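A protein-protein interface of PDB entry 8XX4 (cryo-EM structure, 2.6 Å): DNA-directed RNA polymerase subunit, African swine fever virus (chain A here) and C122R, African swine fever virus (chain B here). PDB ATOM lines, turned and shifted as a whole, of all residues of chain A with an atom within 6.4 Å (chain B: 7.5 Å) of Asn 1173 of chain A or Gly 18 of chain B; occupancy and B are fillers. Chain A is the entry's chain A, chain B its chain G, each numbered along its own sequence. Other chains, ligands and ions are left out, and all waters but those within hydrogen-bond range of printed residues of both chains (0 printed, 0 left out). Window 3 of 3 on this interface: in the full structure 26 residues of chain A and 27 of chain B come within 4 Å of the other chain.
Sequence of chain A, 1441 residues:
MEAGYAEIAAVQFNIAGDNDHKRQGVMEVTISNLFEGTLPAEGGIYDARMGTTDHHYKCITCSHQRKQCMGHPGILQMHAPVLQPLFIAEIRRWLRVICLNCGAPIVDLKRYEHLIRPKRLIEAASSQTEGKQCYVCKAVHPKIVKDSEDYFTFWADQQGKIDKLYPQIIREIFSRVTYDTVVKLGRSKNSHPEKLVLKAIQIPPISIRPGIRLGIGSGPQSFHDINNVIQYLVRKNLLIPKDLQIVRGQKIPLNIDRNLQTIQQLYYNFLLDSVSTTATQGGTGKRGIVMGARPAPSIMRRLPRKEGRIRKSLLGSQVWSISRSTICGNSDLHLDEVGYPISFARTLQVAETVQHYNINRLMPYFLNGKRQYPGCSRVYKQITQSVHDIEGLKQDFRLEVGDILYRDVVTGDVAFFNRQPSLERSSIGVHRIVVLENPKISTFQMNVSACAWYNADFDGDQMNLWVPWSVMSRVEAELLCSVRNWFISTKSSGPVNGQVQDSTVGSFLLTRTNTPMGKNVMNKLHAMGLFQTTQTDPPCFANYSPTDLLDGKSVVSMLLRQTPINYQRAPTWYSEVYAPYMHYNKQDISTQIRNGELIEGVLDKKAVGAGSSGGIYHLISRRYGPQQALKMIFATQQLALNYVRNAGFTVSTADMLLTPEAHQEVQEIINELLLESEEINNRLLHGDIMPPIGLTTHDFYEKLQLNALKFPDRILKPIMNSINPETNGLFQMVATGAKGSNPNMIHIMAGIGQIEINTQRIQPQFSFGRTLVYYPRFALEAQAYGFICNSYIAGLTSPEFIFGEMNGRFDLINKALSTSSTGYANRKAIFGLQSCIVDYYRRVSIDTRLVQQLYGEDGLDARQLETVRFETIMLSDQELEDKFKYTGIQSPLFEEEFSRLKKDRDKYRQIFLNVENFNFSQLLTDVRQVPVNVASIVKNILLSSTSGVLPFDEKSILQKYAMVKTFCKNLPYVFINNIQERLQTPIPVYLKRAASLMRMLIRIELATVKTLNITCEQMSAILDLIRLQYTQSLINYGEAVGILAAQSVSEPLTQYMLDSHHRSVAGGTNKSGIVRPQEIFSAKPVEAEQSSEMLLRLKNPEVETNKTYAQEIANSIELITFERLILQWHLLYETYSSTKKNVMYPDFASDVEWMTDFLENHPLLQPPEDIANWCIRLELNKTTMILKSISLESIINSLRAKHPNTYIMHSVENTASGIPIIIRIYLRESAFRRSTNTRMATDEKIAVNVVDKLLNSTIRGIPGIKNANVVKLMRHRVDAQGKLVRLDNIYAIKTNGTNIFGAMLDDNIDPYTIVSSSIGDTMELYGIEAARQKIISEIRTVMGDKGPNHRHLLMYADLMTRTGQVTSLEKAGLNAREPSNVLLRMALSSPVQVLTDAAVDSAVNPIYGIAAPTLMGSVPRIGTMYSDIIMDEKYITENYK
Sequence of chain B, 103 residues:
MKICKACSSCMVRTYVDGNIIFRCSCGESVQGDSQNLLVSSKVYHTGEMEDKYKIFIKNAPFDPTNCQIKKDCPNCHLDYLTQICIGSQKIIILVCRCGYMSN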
ATOM      1  N   LEU A1132      10.097  15.254   8.149  1.00  0.00           N
ATOM      2  CA  LEU A1132      11.063  16.278   7.779  1.00  0.00           C
ATOM      3  C   LEU A1132      11.321  17.209   8.954  1.00  0.00           C
ATOM      4  O   LEU A1132      10.417  17.493   9.744  1.00  0.00           O
ATOM      5  CB  LEU A1132      10.571  17.091   6.580  1.00  0.00           C
ATOM      6  CG  LEU A1132       9.667  16.358   5.597  1.00  0.00           C
ATOM      7  CD1 LEU A1132       9.082  17.325   4.594  1.00  0.00           C
ATOM      8  CD2 LEU A1132      10.457  15.280   4.888  1.00  0.00           C
ATOM      9  N   TYR A1133      12.560  17.687   9.056  1.00  0.00           N
ATOM     10  CA  TYR A1133      12.912  18.649  10.091  1.00  0.00           C
ATOM     11  C   TYR A1133      12.426  20.058   9.783  1.00  0.00           C
ATOM     12  O   TYR A1133      12.536  20.931  10.648  1.00  0.00           O
ATOM     13  CB  TYR A1133      14.426  18.673  10.306  1.00  0.00           C
ATOM     14  CG  TYR A1133      14.816  19.220  11.655  1.00  0.00           C
ATOM     15  CD1 TYR A1133      14.357  18.628  12.822  1.00  0.00           C
ATOM     16  CD2 TYR A1133      15.616  20.350  11.764  1.00  0.00           C
ATOM     17  CE1 TYR A1133      14.697  19.135  14.058  1.00  0.00           C
ATOM     18  CE2 TYR A1133      15.961  20.862  12.994  1.00  0.00           C
ATOM     19  CZ  TYR A1133      15.498  20.251  14.139  1.00  0.00           C
ATOM     20  OH  TYR A1133      15.837  20.753  15.375  1.00  0.00           O
ATOM     21  N   GLU A1134      11.897  20.299   8.589  1.00  0.00           N
ATOM     22  CA  GLU A1134      11.537  21.648   8.184  1.00  0.00           C
ATOM     23  C   GLU A1134      10.368  22.184   9.004  1.00  0.00           C
ATOM     24  O   GLU A1134       9.510  21.433   9.475  1.00  0.00           O
ATOM     25  CB  GLU A1134      11.188  21.681   6.698  1.00  0.00           C
ATOM     26  CG  GLU A1134      10.037  20.778   6.308  1.00  0.00           C
ATOM     27  CD  GLU A1134       9.820  20.740   4.811  1.00  0.00           C
ATOM     28  OE1 GLU A1134      10.801  20.932   4.067  1.00  0.00           O
ATOM     29  OE2 GLU A1134       8.671  20.524   4.375  1.00  0.00           O
ATOM     30  N   THR A1135      10.346  23.499   9.168  1.00  0.00           N
ATOM     31  CA  THR A1135       9.277  24.223   9.843  1.00  0.00           C
ATOM     32  C   THR A1135       8.561  25.118   8.837  1.00  0.00           C
ATOM     33  O   THR A1135       8.950  25.216   7.670  1.00  0.00           O
ATOM     34  CB  THR A1135       9.826  25.043  11.014  1.00  0.00           C
ATOM     35  OG1 THR A1135       8.762  25.372  11.915  1.00  0.00           O
ATOM     36  CG2 THR A1135      10.478  26.320  10.514  1.00  0.00           C
ATOM     37  N   TYR A1136       7.501  25.777   9.297  1.00  0.00           N
ATOM     38  CA  TYR A1136       6.734  26.684   8.458  1.00  0.00           C
ATOM     39  C   TYR A1136       6.493  27.992   9.196  1.00  0.00           C
ATOM     40  O   TYR A1136       6.349  28.018  10.421  1.00  0.00           O
ATOM     41  CB  TYR A1136       5.398  26.067   8.040  1.00  0.00           C
ATOM     42  CG  TYR A1136       4.809  26.690   6.798  1.00  0.00           C
ATOM     43  CD1 TYR A1136       5.584  26.878   5.665  1.00  0.00           C
ATOM     44  CD2 TYR A1136       3.478  27.078   6.753  1.00  0.00           C
ATOM     45  CE1 TYR A1136       5.057  27.445   4.525  1.00  0.00           C
ATOM     46  CE2 TYR A1136       2.939  27.644   5.615  1.00  0.00           C
ATOM     47  CZ  TYR A1136       3.734  27.824   4.504  1.00  0.00           C
ATOM     48  OH  TYR A1136       3.208  28.387   3.363  1.00  0.00           O
ATOM     49  N   VAL A1143      12.851  27.603   5.575  1.00  0.00           N
ATOM     50  CA  VAL A1143      13.644  26.595   4.881  1.00  0.00           C
ATOM     51  C   VAL A1143      12.784  25.364   4.629  1.00  0.00           C
ATOM     52  O   VAL A1143      12.081  24.883   5.526  1.00  0.00           O
ATOM     53  CB  VAL A1143      14.898  26.243   5.694  1.00  0.00           C
ATOM     54  CG1 VAL A1143      15.765  25.250   4.934  1.00  0.00           C
ATOM     55  CG2 VAL A1143      15.681  27.503   6.029  1.00  0.00           C
ATOM     56  N   ILE A1171       5.301  27.162  16.718  1.00  0.00           N
ATOM     57  CA  ILE A1171       5.433  25.949  15.920  1.00  0.00           C
ATOM     58  C   ILE A1171       6.848  25.395  16.034  1.00  0.00           C
ATOM     59  O   ILE A1171       7.831  26.147  16.104  1.00  0.00           O
ATOM     60  CB  ILE A1171       5.050  26.240  14.458  1.00  0.00           C
ATOM     61  CG1 ILE A1171       4.873  24.941  13.672  1.00  0.00           C
ATOM     62  CG2 ILE A1171       6.076  27.144  13.792  1.00  0.00           C
ATOM     63  CD1 ILE A1171       4.473  25.166  12.236  1.00  0.00           C
ATOM     64  N   ALA A1172       6.956  24.070  16.081  1.00  0.00           N
ATOM     65  CA  ALA A1172       8.236  23.406  16.263  1.00  0.00           C
ATOM     66  C   ALA A1172       8.867  23.060  14.915  1.00  0.00           C
ATOM     67  O   ALA A1172       8.216  23.070  13.869  1.00  0.00           O
ATOM     68  CB  ALA A1172       8.073  22.150  17.116  1.00  0.00           C
ATOM     69  N   ASN A1173      10.159  22.743  14.956  1.00  0.00           N
ATOM     70  CA  ASN A1173      10.931  22.474  13.743  1.00  0.00           C
ATOM     71  C   ASN A1173      10.852  20.991  13.376  1.00  0.00           C
ATOM     72  O   ASN A1173      11.836  20.257  13.396  1.00  0.00           O
ATOM     73  CB  ASN A1173      12.374  22.924  13.928  1.00  0.00           C
ATOM     74  CG  ASN A1173      12.855  23.820  12.807  1.00  0.00           C
ATOM     75  OD1 ASN A1173      12.699  23.502  11.631  1.00  0.00           O
ATOM     76  ND2 ASN A1173      13.443  24.952  13.170  1.00  0.00           N
ATOM     77  N   TRP A1174       9.639  20.562  13.039  1.00  0.00           N
ATOM     78  CA  TRP A1174       9.385  19.198  12.603  1.00  0.00           C
ATOM     79  C   TRP A1174       8.189  19.212  11.667  1.00  0.00           C
ATOM     80  O   TRP A1174       7.386  20.147  11.673  1.00  0.00           O
ATOM     81  CB  TRP A1174       9.117  18.256  13.782  1.00  0.00           C
ATOM     82  CG  TRP A1174      10.315  17.968  14.621  1.00  0.00           C
ATOM     83  CD1 TRP A1174      10.639  18.549  15.808  1.00  0.00           C
ATOM     84  CD2 TRP A1174      11.349  17.021  14.341  1.00  0.00           C
ATOM     85  NE1 TRP A1174      11.812  18.024  16.289  1.00  0.00           N
ATOM     86  CE2 TRP A1174      12.270  17.083  15.405  1.00  0.00           C
ATOM     87  CE3 TRP A1174      11.588  16.128  13.294  1.00  0.00           C
ATOM     88  CZ2 TRP A1174      13.409  16.287  15.451  1.00  0.00           C
ATOM     89  CZ3 TRP A1174      12.717  15.338  13.343  1.00  0.00           C
ATOM     90  CH2 TRP A1174      13.615  15.422  14.413  1.00  0.00           C
ATOM     91  N   CYS A1175       8.074  18.165  10.858  1.00  0.00           N
ATOM     92  CA  CYS A1175       6.949  18.062   9.943  1.00  0.00           C
ATOM     93  C   CYS A1175       6.727  16.603   9.587  1.00  0.00           C
ATOM     94  O   CYS A1175       7.623  15.767   9.714  1.00  0.00           O
ATOM     95  CB  CYS A1175       7.175  18.891   8.675  1.00  0.00           C
ATOM     96  SG  CYS A1175       5.765  18.922   7.553  1.00  0.00           S
ATOM     97  N   LEU A1227       4.325  19.359  14.696  1.00  0.00           N
ATOM     98  CA  LEU A1227       4.214  19.316  16.146  1.00  0.00           C
ATOM     99  C   LEU A1227       4.275  20.736  16.695  1.00  0.00           C
ATOM    100  O   LEU A1227       5.042  21.569  16.207  1.00  0.00           O
ATOM    101  CB  LEU A1227       5.336  18.459  16.734  1.00  0.00           C
ATOM    102  CG  LEU A1227       5.391  16.975  16.351  1.00  0.00           C
ATOM    103  CD1 LEU A1227       5.999  16.751  14.974  1.00  0.00           C
ATOM    104  CD2 LEU A1227       6.180  16.207  17.390  1.00  0.00           C
ATOM    105  N   ARG A1228       3.454  21.022  17.707  1.00  0.00           N
ATOM    106  CA  ARG A1228       3.269  22.416  18.088  1.00  0.00           C
ATOM    107  C   ARG A1228       4.474  22.961  18.845  1.00  0.00           C
ATOM    108  O   ARG A1228       5.326  23.625  18.250  1.00  0.00           O
ATOM    109  CB  ARG A1228       2.005  22.521  18.948  1.00  0.00           C
ATOM    110  CG  ARG A1228       0.748  22.972  18.225  1.00  0.00           C
ATOM    111  CD  ARG A1228      -0.166  23.760  19.157  1.00  0.00           C
ATOM    112  NE  ARG A1228      -1.035  24.696  18.454  1.00  0.00           N
ATOM    113  CZ  ARG A1228      -0.739  25.969  18.236  1.00  0.00           C
ATOM    114  NH1 ARG A1228       0.323  26.533  18.787  1.00  0.00           N
ATOM    115  NH2 ARG A1228      -1.550  26.704  17.483  1.00  0.00           N
ATOM    116  N   PHE A1232       7.295  17.833  22.985  1.00  0.00           N
ATOM    117  CA  PHE A1232       8.617  17.675  23.584  1.00  0.00           C
ATOM    118  C   PHE A1232       8.555  18.232  25.001  1.00  0.00           C
ATOM    119  O   PHE A1232       8.577  19.449  25.201  1.00  0.00           O
ATOM    120  CB  PHE A1232       9.676  18.378  22.742  1.00  0.00           C
ATOM    121  CG  PHE A1232       9.437  18.268  21.265  1.00  0.00           C
ATOM    122  CD1 PHE A1232       9.832  17.139  20.571  1.00  0.00           C
ATOM    123  CD2 PHE A1232       8.806  19.285  20.574  1.00  0.00           C
ATOM    124  CE1 PHE A1232       9.608  17.031  19.217  1.00  0.00           C
ATOM    125  CE2 PHE A1232       8.578  19.181  19.222  1.00  0.00           C
ATOM    126  CZ  PHE A1232       8.979  18.052  18.544  1.00  0.00           C
ATOM    127  N   TYR B  15      20.033  17.120  15.459  1.00  0.00           N
ATOM    128  CA  TYR B  15      19.232  18.267  15.043  1.00  0.00           C
ATOM    129  C   TYR B  15      19.111  19.315  16.143  1.00  0.00           C
ATOM    130  O   TYR B  15      18.017  19.538  16.670  1.00  0.00           O
ATOM    131  CB  TYR B  15      17.827  17.820  14.640  1.00  0.00           C
ATOM    132  CG  TYR B  15      17.774  16.606  13.752  1.00  0.00           C
ATOM    133  CD1 TYR B  15      17.760  15.333  14.290  1.00  0.00           C
ATOM    134  CD2 TYR B  15      17.701  16.737  12.378  1.00  0.00           C
ATOM    135  CE1 TYR B  15      17.706  14.228  13.486  1.00  0.00           C
ATOM    136  CE2 TYR B  15      17.646  15.635  11.559  1.00  0.00           C
ATOM    137  CZ  TYR B  15      17.644  14.380  12.118  1.00  0.00           C
ATOM    138  OH  TYR B  15      17.587  13.270  11.307  1.00  0.00           O
ATOM    139  N   VAL B  16      20.216  19.966  16.500  1.00  0.00           N
ATOM    140  CA  VAL B  16      20.227  20.983  17.545  1.00  0.00           C
ATOM    141  C   VAL B  16      20.856  22.251  16.983  1.00  0.00           C
ATOM    142  O   VAL B  16      21.996  22.225  16.509  1.00  0.00           O
ATOM    143  CB  VAL B  16      20.988  20.513  18.800  1.00  0.00           C
ATOM    144  CG1 VAL B  16      20.763  21.479  19.951  1.00  0.00           C
ATOM    145  CG2 VAL B  16      20.550  19.110  19.198  1.00  0.00           C
ATOM    146  N   ASP B  17      20.116  23.356  17.039  1.00  0.00           N
ATOM    147  CA  ASP B  17      18.758  23.391  17.571  1.00  0.00           C
ATOM    148  C   ASP B  17      17.750  23.622  16.453  1.00  0.00           C
ATOM    149  O   ASP B  17      16.783  22.875  16.314  1.00  0.00           O
ATOM    150  CB  ASP B  17      18.622  24.474  18.649  1.00  0.00           C
ATOM    151  CG  ASP B  17      19.299  25.777  18.263  1.00  0.00           C
ATOM    152  OD1 ASP B  17      19.547  25.994  17.059  1.00  0.00           O
ATOM    153  OD2 ASP B  17      19.583  26.589  19.170  1.00  0.00           O
ATOM    154  N   GLY B  18      17.985  24.660  15.656  1.00  0.00           N
ATOM    155  CA  GLY B  18      17.154  24.977  14.517  1.00  0.00           C
ATOM    156  C   GLY B  18      17.661  24.473  13.187  1.00  0.00           C
ATOM    157  O   GLY B  18      17.045  24.759  12.157  1.00  0.00           O
ATOM    158  N   ASN B  19      18.762  23.728  13.173  1.00  0.00           N
ATOM    159  CA  ASN B  19      19.374  23.261  11.938  1.00  0.00           C
ATOM    160  C   ASN B  19      19.882  21.840  12.158  1.00  0.00           C
ATOM    161  O   ASN B  19      19.570  21.194  13.164  1.00  0.00           O
ATOM    162  CB  ASN B  19      20.490  24.218  11.499  1.00  0.00           C
ATOM    163  CG  ASN B  19      21.410  24.596  12.640  1.00  0.00           C
ATOM    164  OD1 ASN B  19      21.105  24.351  13.807  1.00  0.00           O
ATOM    165  ND2 ASN B  19      22.543  25.204  12.310  1.00  0.00           N
ATOM    166  N   ILE B  20      20.679  21.354  11.212  1.00  0.00           N
ATOM    167  CA  ILE B  20      21.201  19.993  11.223  1.00  0.00           C
ATOM    168  C   ILE B  20      22.719  20.062  11.320  1.00  0.00           C
ATOM    169  O   ILE B  20      23.376  20.632  10.441  1.00  0.00           O
ATOM    170  CB  ILE B  20      20.766  19.217   9.972  1.00  0.00           C
ATOM    171  CG1 ILE B  20      20.704  20.158   8.770  1.00  0.00           C
ATOM    172  CG2 ILE B  20      19.418  18.579  10.186  1.00  0.00           C
ATOM    173  CD1 ILE B  20      20.582  19.450   7.456  1.00  0.00           C
ATOM    174  N   ASP B  33      22.556  21.025   4.353  1.00  0.00           N
ATOM    175  CA  ASP B  33      21.189  21.531   4.314  1.00  0.00           C
ATOM    176  C   ASP B  33      20.402  20.753   3.265  1.00  0.00           C
ATOM    177  O   ASP B  33      20.861  19.729   2.751  1.00  0.00           O
ATOM    178  CB  ASP B  33      21.171  23.038   4.028  1.00  0.00           C
ATOM    179  CG  ASP B  33      21.602  23.869   5.223  1.00  0.00           C
ATOM    180  OD1 ASP B  33      21.012  23.698   6.310  1.00  0.00           O
ATOM    181  OD2 ASP B  33      22.528  24.692   5.073  1.00  0.00           O
ATOM    182  N   LEU B  37      17.450  17.034   5.395  1.00  0.00           N
ATOM    183  CA  LEU B  37      16.362  17.343   6.313  1.00  0.00           C
ATOM    184  C   LEU B  37      15.290  16.261   6.371  1.00  0.00           C
ATOM    185  O   LEU B  37      14.334  16.404   7.138  1.00  0.00           O
ATOM    186  CB  LEU B  37      15.717  18.681   5.936  1.00  0.00           C
ATOM    187  CG  LEU B  37      16.566  19.931   6.170  1.00  0.00           C
ATOM    188  CD1 LEU B  37      16.201  21.016   5.174  1.00  0.00           C
ATOM    189  CD2 LEU B  37      16.420  20.434   7.597  1.00  0.00           C
ATOM    190  N   VAL B  39      14.284  13.264   7.899  1.00  0.00           N
ATOM    191  CA  VAL B  39      14.686  12.448   9.040  1.00  0.00           C
ATOM    192  C   VAL B  39      14.346  10.984   8.800  1.00  0.00           C
ATOM    193  O   VAL B  39      15.185  10.095   8.981  1.00  0.00           O
ATOM    194  CB  VAL B  39      14.028  12.977  10.323  1.00  0.00           C
ATOM    195  CG1 VAL B  39      14.351  12.072  11.490  1.00  0.00           C
ATOM    196  CG2 VAL B  39      14.487  14.393  10.588  1.00  0.00           C
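Printed residues of chain B within 4 Å of Leu 1132 of chain A: Leu 37. Tyr 1136 of chain A touches none of the printed residues of chain B. Of chain B, only Gly 18 (3.7 Å) comes within 4 Å of Asn 1173 of chain A. Cys 1175 of chain A touches none of the printed residues of chain B. Of the printed residues of chain A, Asp 17 of chain B touches Tyr 1133. Of the printed residues of chain A, Gly 18 of chain B touches Tyr 1133 (3.996 Å) and Asn 1173 (3.7 Å). Printed residues of chain A within 4 Å of Leu 37 of chain B: Leu 1132 and Tyr 1133. Printed residues of chain A within 4 Å of Val 39 of chain B: Trp 1174. The nearest printed residue of chain A that does not touch Gly 18 of chain B is Val 1143 of chain A (6.9 Å). The nearest printed residue of chain B that does not touch Tyr 1133 of chain A is Val 39 of chain B (4.1 Å).
The backbone carbonyl oxygen of Tyr 15 of chain B is in hydrogen-bond range of the side-chain hydroxyl of Tyr 1133 of chain A, 2.8 Å away. The side-chain hydroxyl of Tyr 1133 of chain A lies within hydrogen-bond range of the backbone carbonyl oxygen of Asp 17 of chain B (2.5 Å). O of Leu 37 of chain B lies within hydrogen-bond range of N of Tyr 1133 of chain A, at 2.9 Å.
Of the 9 printed residues of chain B, 6 touch a printed residue of chain A. Hydrophobic or aromatic side chains of chain B within 4 Å of the printed part of chain A: Tyr 15, Leu 37 and Val 39. Of the 14 printed residues of chain A, 4 touch a printed residue of chain B. Hydrophobic or aromatic side chains of chain A within 4 Å of the printed part of chain B: Leu 1132, Tyr 1133 and Trp 1174. Among the printed residues, 8 pairs touch across the chains.
Among the printed residues, pairs that only touch across the chains: Leu 1132 of chain A with Leu 37 of chain B (3.3 Å), Trp 1174 of chain A with Val 39 of chain B (3.4 Å), Tyr 1133 of chain A with Asn 19 of chain B (3.6 Å), Asn 1173 of chain A with Gly 18 of chain B (3.7 Å) and Tyr 1133 of chain A with Gly 18 of chain B (3.996 Å).
The backbone NH (N) of Cys 1175 of chain A is in hydrogen-bond range of the backbone carbonyl oxygen (O) of Leu 1132 of chain A, 2.7 Å away. The backbone carbonyl oxygen (O) of Tyr 1133 of chain A lies close to the side-chain amide oxygen (OD1) of Asn 1173 of chain A (2.8 Å). N of Thr 1135 of chain A sits close to OD1 of Asn 1173 of chain A (3.4 Å).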
